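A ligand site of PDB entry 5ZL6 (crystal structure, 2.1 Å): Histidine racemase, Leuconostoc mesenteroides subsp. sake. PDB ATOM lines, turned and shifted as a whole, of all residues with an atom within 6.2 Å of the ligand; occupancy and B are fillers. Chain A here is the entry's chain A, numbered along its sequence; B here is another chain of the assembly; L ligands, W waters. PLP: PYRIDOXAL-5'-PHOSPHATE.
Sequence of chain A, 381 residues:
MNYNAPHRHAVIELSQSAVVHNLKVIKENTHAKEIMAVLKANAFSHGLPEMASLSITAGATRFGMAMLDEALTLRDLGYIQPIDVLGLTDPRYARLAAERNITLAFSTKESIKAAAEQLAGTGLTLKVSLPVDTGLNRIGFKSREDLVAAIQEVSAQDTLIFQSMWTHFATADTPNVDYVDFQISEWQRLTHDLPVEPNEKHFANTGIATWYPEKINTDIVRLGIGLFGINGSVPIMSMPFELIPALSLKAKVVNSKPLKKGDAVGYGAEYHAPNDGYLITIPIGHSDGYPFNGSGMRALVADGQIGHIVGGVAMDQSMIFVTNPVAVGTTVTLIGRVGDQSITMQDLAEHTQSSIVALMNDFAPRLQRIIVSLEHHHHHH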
ATOM      1  N   VAL A  38     -12.916 -18.901  18.453  1.00  0.00           N
ATOM      2  CA  VAL A  38     -12.418 -18.021  19.505  1.00  0.00           C
ATOM      3  C   VAL A  38     -12.461 -16.586  19.011  1.00  0.00           C
ATOM      4  O   VAL A  38     -11.638 -16.177  18.199  1.00  0.00           O
ATOM      5  CB  VAL A  38     -10.984 -18.395  19.942  1.00  0.00           C
ATOM      6  CG1 VAL A  38     -10.535 -17.506  21.094  1.00  0.00           C
ATOM      7  CG2 VAL A  38     -10.910 -19.867  20.344  1.00  0.00           C
ATOM      8  N   LYS A  40     -12.482 -13.726  20.965  1.00  0.00           N
ATOM      9  CA  LYS A  40     -12.137 -12.798  22.040  1.00  0.00           C
ATOM     10  C   LYS A  40     -11.622 -11.481  21.484  1.00  0.00           C
ATOM     11  O   LYS A  40     -11.162 -11.414  20.346  1.00  0.00           O
ATOM     12  CB  LYS A  40     -11.090 -13.427  22.963  1.00  0.00           C
ATOM     13  CG  LYS A  40      -9.741 -13.661  22.298  1.00  0.00           C
ATOM     14  CD  LYS A  40      -8.948 -14.710  23.041  1.00  0.00           C
ATOM     15  CE  LYS A  40      -7.536 -14.812  22.517  1.00  0.00           C
ATOM     16  NZ  LYS A  40      -6.800 -15.948  23.145  1.00  0.00           N
ATOM     17  N   PHE A  44     -10.723 -10.625  17.604  1.00  0.00           N
ATOM     18  CA  PHE A  44      -9.385 -10.195  17.191  1.00  0.00           C
ATOM     19  C   PHE A  44      -9.436  -8.813  16.507  1.00  0.00           C
ATOM     20  O   PHE A  44      -8.687  -8.537  15.576  1.00  0.00           O
ATOM     21  CB  PHE A  44      -8.748 -11.231  16.245  1.00  0.00           C
ATOM     22  CG  PHE A  44      -8.254 -12.477  16.938  1.00  0.00           C
ATOM     23  CD1 PHE A  44      -9.131 -13.317  17.611  1.00  0.00           C
ATOM     24  CD2 PHE A  44      -6.899 -12.816  16.903  1.00  0.00           C
ATOM     25  CE1 PHE A  44      -8.674 -14.467  18.234  1.00  0.00           C
ATOM     26  CE2 PHE A  44      -6.443 -13.962  17.540  1.00  0.00           C
ATOM     27  CZ  PHE A  44      -7.330 -14.785  18.201  1.00  0.00           C
ATOM     28  N   LEU A  86     -12.555 -18.654  28.553  1.00  0.00           N
ATOM     29  CA  LEU A  86     -11.267 -19.310  28.641  1.00  0.00           C
ATOM     30  C   LEU A  86     -10.312 -18.545  29.557  1.00  0.00           C
ATOM     31  O   LEU A  86      -9.170 -18.944  29.765  1.00  0.00           O
ATOM     32  CB  LEU A  86     -10.654 -19.479  27.245  1.00  0.00           C
ATOM     33  CG  LEU A  86     -11.388 -20.411  26.280  1.00  0.00           C
ATOM     34  CD1 LEU A  86     -10.704 -20.447  24.922  1.00  0.00           C
ATOM     35  CD2 LEU A  86     -11.476 -21.823  26.863  1.00  0.00           C
ATOM     36  N   ARG A 138       0.390 -19.274  32.220  1.00  0.00           N
ATOM     37  CA  ARG A 138      -0.466 -18.113  32.443  1.00  0.00           C
ATOM     38  C   ARG A 138      -1.552 -18.431  33.471  1.00  0.00           C
ATOM     39  O   ARG A 138      -1.706 -17.706  34.445  1.00  0.00           O
ATOM     40  CB  ARG A 138      -1.080 -17.613  31.124  1.00  0.00           C
ATOM     41  CG  ARG A 138      -1.927 -18.605  30.373  1.00  0.00           C
ATOM     42  CD  ARG A 138      -3.294 -18.019  30.018  1.00  0.00           C
ATOM     43  NE  ARG A 138      -3.251 -17.109  28.875  1.00  0.00           N
ATOM     44  CZ  ARG A 138      -3.699 -17.420  27.661  1.00  0.00           C
ATOM     45  NH1 ARG A 138      -4.214 -18.617  27.421  1.00  0.00           N
ATOM     46  NH2 ARG A 138      -3.633 -16.517  26.675  1.00  0.00           N
ATOM     47  N   TRP A 166      -8.774 -28.765  29.909  1.00  0.00           N
ATOM     48  CA  TRP A 166      -8.070 -28.324  28.706  1.00  0.00           C
ATOM     49  C   TRP A 166      -6.722 -27.720  29.037  1.00  0.00           C
ATOM     50  O   TRP A 166      -6.448 -27.366  30.180  1.00  0.00           O
ATOM     51  CB  TRP A 166      -8.929 -27.331  27.934  1.00  0.00           C
ATOM     52  CG  TRP A 166      -9.360 -26.101  28.704  1.00  0.00           C
ATOM     53  CD1 TRP A 166     -10.502 -25.954  29.458  1.00  0.00           C
ATOM     54  CD2 TRP A 166      -8.682 -24.839  28.765  1.00  0.00           C
ATOM     55  NE1 TRP A 166     -10.558 -24.695  29.995  1.00  0.00           N
ATOM     56  CE2 TRP A 166      -9.459 -23.980  29.584  1.00  0.00           C
ATOM     57  CE3 TRP A 166      -7.500 -24.345  28.224  1.00  0.00           C
ATOM     58  CZ2 TRP A 166      -9.081 -22.673  29.859  1.00  0.00           C
ATOM     59  CZ3 TRP A 166      -7.121 -23.043  28.508  1.00  0.00           C
ATOM     60  CH2 TRP A 166      -7.915 -22.225  29.316  1.00  0.00           C
ATOM     61  N   THR A 167      -5.852 -27.610  28.028  1.00  0.00           N
ATOM     62  CA  THR A 167      -4.605 -26.877  28.185  1.00  0.00           C
ATOM     63  C   THR A 167      -4.284 -26.119  26.894  1.00  0.00           C
ATOM     64  O   THR A 167      -4.863 -26.381  25.842  1.00  0.00           O
ATOM     65  CB  THR A 167      -3.435 -27.805  28.574  1.00  0.00           C
ATOM     66  OG1 THR A 167      -2.310 -27.012  28.955  1.00  0.00           O
ATOM     67  CG2 THR A 167      -3.041 -28.716  27.424  1.00  0.00           C
ATOM     68  N   HIS A 168      -3.353 -25.170  26.983  1.00  0.00           N
ATOM     69  CA  HIS A 168      -3.038 -24.275  25.875  1.00  0.00           C
ATOM     70  C   HIS A 168      -1.539 -24.280  25.574  1.00  0.00           C
ATOM     71  O   HIS A 168      -0.724 -24.274  26.492  1.00  0.00           O
ATOM     72  CB  HIS A 168      -3.529 -22.862  26.199  1.00  0.00           C
ATOM     73  CG  HIS A 168      -3.557 -21.936  25.023  1.00  0.00           C
ATOM     74  ND1 HIS A 168      -4.174 -22.260  23.834  1.00  0.00           N
ATOM     75  CD2 HIS A 168      -3.082 -20.675  24.864  1.00  0.00           C
ATOM     76  CE1 HIS A 168      -4.064 -21.249  22.987  1.00  0.00           C
ATOM     77  NE2 HIS A 168      -3.408 -20.279  23.597  1.00  0.00           N
ATOM     78  N   ASP A 173       3.049 -22.713  17.424  1.00  0.00           N
ATOM     79  CA  ASP A 173       3.052 -21.611  16.508  1.00  0.00           C
ATOM     80  C   ASP A 173       4.388 -21.510  15.781  1.00  0.00           C
ATOM     81  O   ASP A 173       4.682 -20.494  15.146  1.00  0.00           O
ATOM     82  CB  ASP A 173       2.809 -20.339  17.303  1.00  0.00           C
ATOM     83  CG  ASP A 173       1.847 -19.437  16.658  1.00  0.00           C
ATOM     84  OD1 ASP A 173       1.271 -19.880  15.641  1.00  0.00           O
ATOM     85  OD2 ASP A 173       1.659 -18.310  17.149  1.00  0.00           O
ATOM     86  N   ALA A 204      -6.222 -28.076  21.169  1.00  0.00           N
ATOM     87  CA  ALA A 204      -5.637 -27.489  19.963  1.00  0.00           C
ATOM     88  C   ALA A 204      -6.038 -26.042  19.692  1.00  0.00           C
ATOM     89  O   ALA A 204      -7.213 -25.702  19.705  1.00  0.00           O
ATOM     90  CB  ALA A 204      -5.998 -28.348  18.767  1.00  0.00           C
ATOM     91  N   ASN A 205      -5.035 -25.199  19.451  1.00  0.00           N
ATOM     92  CA  ASN A 205      -5.242 -23.882  18.864  1.00  0.00           C
ATOM     93  C   ASN A 205      -4.899 -23.934  17.377  1.00  0.00           C
ATOM     94  O   ASN A 205      -4.665 -25.014  16.829  1.00  0.00           O
ATOM     95  CB  ASN A 205      -4.400 -22.812  19.579  1.00  0.00           C
ATOM     96  CG  ASN A 205      -2.907 -23.116  19.535  1.00  0.00           C
ATOM     97  OD1 ASN A 205      -2.475 -24.036  18.850  1.00  0.00           O
ATOM     98  ND2 ASN A 205      -2.127 -22.324  20.268  1.00  0.00           N
ATOM     99  N   THR A 206      -4.876 -22.769  16.737  1.00  0.00           N
ATOM    100  CA  THR A 206      -4.600 -22.707  15.306  1.00  0.00           C
ATOM    101  C   THR A 206      -3.286 -23.401  14.980  1.00  0.00           C
ATOM    102  O   THR A 206      -3.216 -24.207  14.056  1.00  0.00           O
ATOM    103  CB  THR A 206      -4.533 -21.260  14.802  1.00  0.00           C
ATOM    104  OG1 THR A 206      -5.844 -20.676  14.858  1.00  0.00           O
ATOM    105  CG2 THR A 206      -4.037 -21.206  13.367  1.00  0.00           C
ATOM    106  N   GLY A 207      -2.252 -23.099  15.766  1.00  0.00           N
ATOM    107  CA  GLY A 207      -0.934 -23.669  15.545  1.00  0.00           C
ATOM    108  C   GLY A 207      -0.944 -25.186  15.533  1.00  0.00           C
ATOM    109  O   GLY A 207      -0.454 -25.819  14.594  1.00  0.00           O
ATOM    110  N   ARG A 222      -9.859 -25.207  19.216  1.00  0.00           N
ATOM    111  CA  ARG A 222     -10.105 -23.827  19.623  1.00  0.00           C
ATOM    112  C   ARG A 222      -9.462 -22.880  18.620  1.00  0.00           C
ATOM    113  O   ARG A 222      -8.302 -22.502  18.763  1.00  0.00           O
ATOM    114  CB  ARG A 222      -9.591 -23.567  21.035  1.00  0.00           C
ATOM    115  CG  ARG A 222     -10.142 -24.546  22.062  1.00  0.00           C
ATOM    116  CD  ARG A 222      -9.923 -24.068  23.486  1.00  0.00           C
ATOM    117  NE  ARG A 222      -8.509 -23.866  23.780  1.00  0.00           N
ATOM    118  CZ  ARG A 222      -7.707 -24.815  24.269  1.00  0.00           C
ATOM    119  NH1 ARG A 222      -8.164 -26.021  24.516  1.00  0.00           N
ATOM    120  NH2 ARG A 222      -6.429 -24.528  24.503  1.00  0.00           N
ATOM    121  N   LEU A 223     -10.243 -22.498  17.611  1.00  0.00           N
ATOM    122  CA  LEU A 223      -9.717 -21.779  16.450  1.00  0.00           C
ATOM    123  C   LEU A 223      -9.856 -20.264  16.571  1.00  0.00           C
ATOM    124  O   LEU A 223     -10.956 -19.719  16.455  1.00  0.00           O
ATOM    125  CB  LEU A 223     -10.425 -22.262  15.186  1.00  0.00           C
ATOM    126  CG  LEU A 223      -9.877 -21.747  13.860  1.00  0.00           C
ATOM    127  CD1 LEU A 223      -8.428 -22.168  13.694  1.00  0.00           C
ATOM    128  CD2 LEU A 223     -10.723 -22.241  12.702  1.00  0.00           C
ATOM    129  N   GLY A 224      -8.734 -19.602  16.797  1.00  0.00           N
ATOM    130  CA  GLY A 224      -8.710 -18.155  16.814  1.00  0.00           C
ATOM    131  C   GLY A 224      -8.166 -17.572  15.528  1.00  0.00           C
ATOM    132  O   GLY A 224      -8.907 -17.342  14.568  1.00  0.00           O
ATOM    133  N   ILE A 225      -6.858 -17.358  15.489  1.00  0.00           N
ATOM    134  CA  ILE A 225      -6.225 -16.548  14.442  1.00  0.00           C
ATOM    135  C   ILE A 225      -6.380 -17.102  13.017  1.00  0.00           C
ATOM    136  O   ILE A 225      -6.525 -16.327  12.072  1.00  0.00           O
ATOM    137  CB  ILE A 225      -4.722 -16.337  14.749  1.00  0.00           C
ATOM    138  CG1 ILE A 225      -4.065 -15.436  13.707  1.00  0.00           C
ATOM    139  CG2 ILE A 225      -3.999 -17.675  14.882  1.00  0.00           C
ATOM    140  CD1 ILE A 225      -2.642 -15.060  14.042  1.00  0.00           C
ATOM    141  N   GLY A 226      -6.364 -18.427  12.872  1.00  0.00           N
ATOM    142  CA  GLY A 226      -6.462 -19.047  11.568  1.00  0.00           C
ATOM    143  C   GLY A 226      -7.768 -18.703  10.876  1.00  0.00           C
ATOM    144  O   GLY A 226      -7.852 -18.612   9.641  1.00  0.00           O
ATOM    145  N   TYR B 267       3.991 -17.061  25.319  1.00  0.00           N
ATOM    146  CA  TYR B 267       4.104 -17.552  23.950  1.00  0.00           C
ATOM    147  C   TYR B 267       5.550 -17.547  23.485  1.00  0.00           C
ATOM    148  O   TYR B 267       6.258 -16.558  23.643  1.00  0.00           O
ATOM    149  CB  TYR B 267       3.232 -16.708  23.014  1.00  0.00           C
ATOM    150  CG  TYR B 267       1.759 -16.975  23.169  1.00  0.00           C
ATOM    151  CD1 TYR B 267       1.251 -18.263  23.050  1.00  0.00           C
ATOM    152  CD2 TYR B 267       0.872 -15.946  23.457  1.00  0.00           C
ATOM    153  CE1 TYR B 267      -0.093 -18.517  23.195  1.00  0.00           C
ATOM    154  CE2 TYR B 267      -0.483 -16.186  23.598  1.00  0.00           C
ATOM    155  CZ  TYR B 267      -0.960 -17.476  23.465  1.00  0.00           C
ATOM    156  OH  TYR B 267      -2.304 -17.730  23.610  1.00  0.00           O
ATOM    157  N   MET B 315      -3.031 -11.307  24.370  1.00  0.00           N
ATOM    158  CA  MET B 315      -4.137 -10.453  23.935  1.00  0.00           C
ATOM    159  C   MET B 315      -4.927  -9.912  25.126  1.00  0.00           C
ATOM    160  O   MET B 315      -5.207  -8.708  25.193  1.00  0.00           O
ATOM    161  CB  MET B 315      -5.062 -11.215  22.996  1.00  0.00           C
ATOM    162  CG  MET B 315      -4.549 -11.262  21.560  1.00  0.00           C
ATOM    163  SD  MET B 315      -5.473 -12.376  20.490  1.00  0.00           S
ATOM    164  CE  MET B 315      -7.027 -11.499  20.311  1.00  0.00           C
ATOM    165  N   ASP B 316      -5.256 -10.789  26.060  1.00  0.00           N
ATOM    166  CA  ASP B 316      -6.165 -10.452  27.153  1.00  0.00           C
ATOM    167  C   ASP B 316      -5.526 -10.565  28.541  1.00  0.00           C
ATOM    168  O   ASP B 316      -6.119 -10.162  29.551  1.00  0.00           O
ATOM    169  CB  ASP B 316      -7.398 -11.365  27.089  1.00  0.00           C
ATOM    170  CG  ASP B 316      -7.855 -11.597  25.656  1.00  0.00           C
ATOM    171  OD1 ASP B 316      -8.002 -10.608  24.902  1.00  0.00           O
ATOM    172  OD2 ASP B 316      -8.062 -12.774  25.273  1.00  0.00           O
ATOM    173  N   GLN B 317      -4.315 -11.122  28.610  1.00  0.00           N
ATOM    174  CA  GLN B 317      -3.669 -11.358  29.893  1.00  0.00           C
ATOM    175  C   GLN B 317      -2.179 -11.011  29.862  1.00  0.00           C
ATOM    176  O   GLN B 317      -1.554 -10.992  28.804  1.00  0.00           O
ATOM    177  CB  GLN B 317      -3.857 -12.812  30.318  1.00  0.00           C
ATOM    178  CG  GLN B 317      -5.310 -13.245  30.402  1.00  0.00           C
ATOM    179  CD  GLN B 317      -5.479 -14.744  30.524  1.00  0.00           C
ATOM    180  OE1 GLN B 317      -5.688 -15.439  29.540  1.00  0.00           O
ATOM    181  NE2 GLN B 317      -5.378 -15.238  31.758  1.00  0.00           N
HETATM  182  N1  PLP L   1      -7.449 -21.324  23.480  1.00  0.00           N
HETATM  183  C2  PLP L   1      -7.154 -20.268  24.527  1.00  0.00           C
HETATM  184  C2A PLP L   1      -7.127 -20.641  26.006  1.00  0.00           C
HETATM  185  C3  PLP L   1      -6.887 -18.803  24.091  1.00  0.00           C
HETATM  186  O3  PLP L   1      -6.597 -17.828  25.058  1.00  0.00           O
HETATM  187  C4  PLP L   1      -6.912 -18.440  22.629  1.00  0.00           C
HETATM  188  C4A PLP L   1      -6.665 -16.981  22.203  1.00  0.00           C
HETATM  189  C5  PLP L   1      -7.217 -19.501  21.591  1.00  0.00           C
HETATM  190  C6  PLP L   1      -7.475 -20.956  22.008  1.00  0.00           C
HETATM  191  C5A PLP L   1      -7.141 -19.166  20.107  1.00  0.00           C
HETATM  192  O4P PLP L   1      -5.785 -19.425  19.831  1.00  0.00           O
HETATM  193  P   PLP L   1      -5.187 -19.104  18.323  1.00  0.00           P
HETATM  194  O1P PLP L   1      -3.734 -19.242  18.330  1.00  0.00           O
HETATM  195  O2P PLP L   1      -5.841 -20.201  17.272  1.00  0.00           O
HETATM  196  O3P PLP L   1      -5.596 -17.560  17.923  1.00  0.00           O
HETATM  197  O   HOH W   1      -2.475 -19.388  20.807  1.00  0.00           O
HETATM  198  O   HOH W   2      -1.603 -20.840  16.984  1.00  0.00           O
HETATM  199  O   HOH W   3      -3.706 -15.378  19.343  1.00  0.00           O
HETATM  200  O   HOH W   4      -2.040 -16.882  18.088  1.00  0.00           O
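An oxygen (O2P) of the ligand lies within hydrogen-bond range of the backbone NH of Thr 206 (2.8 Å).
NH1 of Arg 138 lies within hydrogen-bond range of O3 of the ligand, at 3.4 Å.
A nitrogen (N1) of the ligand lies close to a ring nitrogen (ND1) of His 168 (3.4 Å).
An oxygen (O3P) of the ligand is in hydrogen-bond range of the backbone NH (N) of Ile 225 (2.7 Å).
NE of Arg 222 lies within hydrogen-bond range of N1 of the ligand (2.8 Å).
The backbone NH (N) of Gly 224 lies within hydrogen-bond range of an oxygen (O2P) of the ligand (3.0 Å).
O2P of the ligand is in hydrogen-bond range of OG1 of Thr 206 (2.5 Å).
The side-chain amino group (NZ) of Lys 40 is bonded to a carbon (C4A) of the ligand (1.4 Å).
The backbone carbonyl oxygen (O) of Leu 223 lies within hydrogen-bond range of the backbone NH (N) of Val 38 (2.9 Å).
The backbone carbonyl oxygen of Thr 167 lies within hydrogen-bond range of the guanidinium group of Arg 222, at 2.8 Å.
The backbone NH of Gly 226 sits at hydrogen-bond distance from the side-chain hydroxyl of Thr 206, at 3.0 Å.
The side-chain amide oxygen (OD1) of Asn 205 sits close to the backbone NH (N) of Gly 207 (3.2 Å).
The side-chain hydroxyl of Tyr 267 of chain B sits at hydrogen-bond distance from a ring nitrogen (NE2) of His 168, 2.8 Å away.
ND1 of His 168 lies within hydrogen-bond range of NH2 of Arg 222, at 3.3 Å.
NE of Arg 138 lies within hydrogen-bond range of OE1 of Gln 317 of chain B (3.0 Å).
N of Arg 222 sits at hydrogen-bond distance from O of Ala 204.
Merely in contact with the ligand: Phe 44, Trp 166, Leu 86, Asn 205 and Val 38.
Hydrophobic or aromatic side chains within 4 Å of the ligand: Val 38, Phe 44, Leu 86, Trp 166, His 168 and Ile 225.
Within 4 Å of the ligand: Val 38, Lys 40, Phe 44, Leu 86, Arg 138, Trp 166, His 168, Asn 205, Thr 206, Arg 222, Gly 224 and Ile 225.
The nearest printed residue that does not touch the ligand is Leu 223 (4.1 Å).
Water W1 lies within hydrogen-bond range of O1P of the ligand (2.8 Å), ND2 of Asn 205 (3.0 Å), NE2 of His 168 (3.1 Å) and OH of Tyr 267 of chain B (3.3 Å).
Water W2 lies within hydrogen-bond range of the backbone NH (N) of Gly 207, an oxygen (O1P) of the ligand and the side-chain carboxylate (OD1) of Asp 173.
Water W3 bridges O3P of the ligand (3.2 Å) and SD of Met 315 of chain B (3.7 Å).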
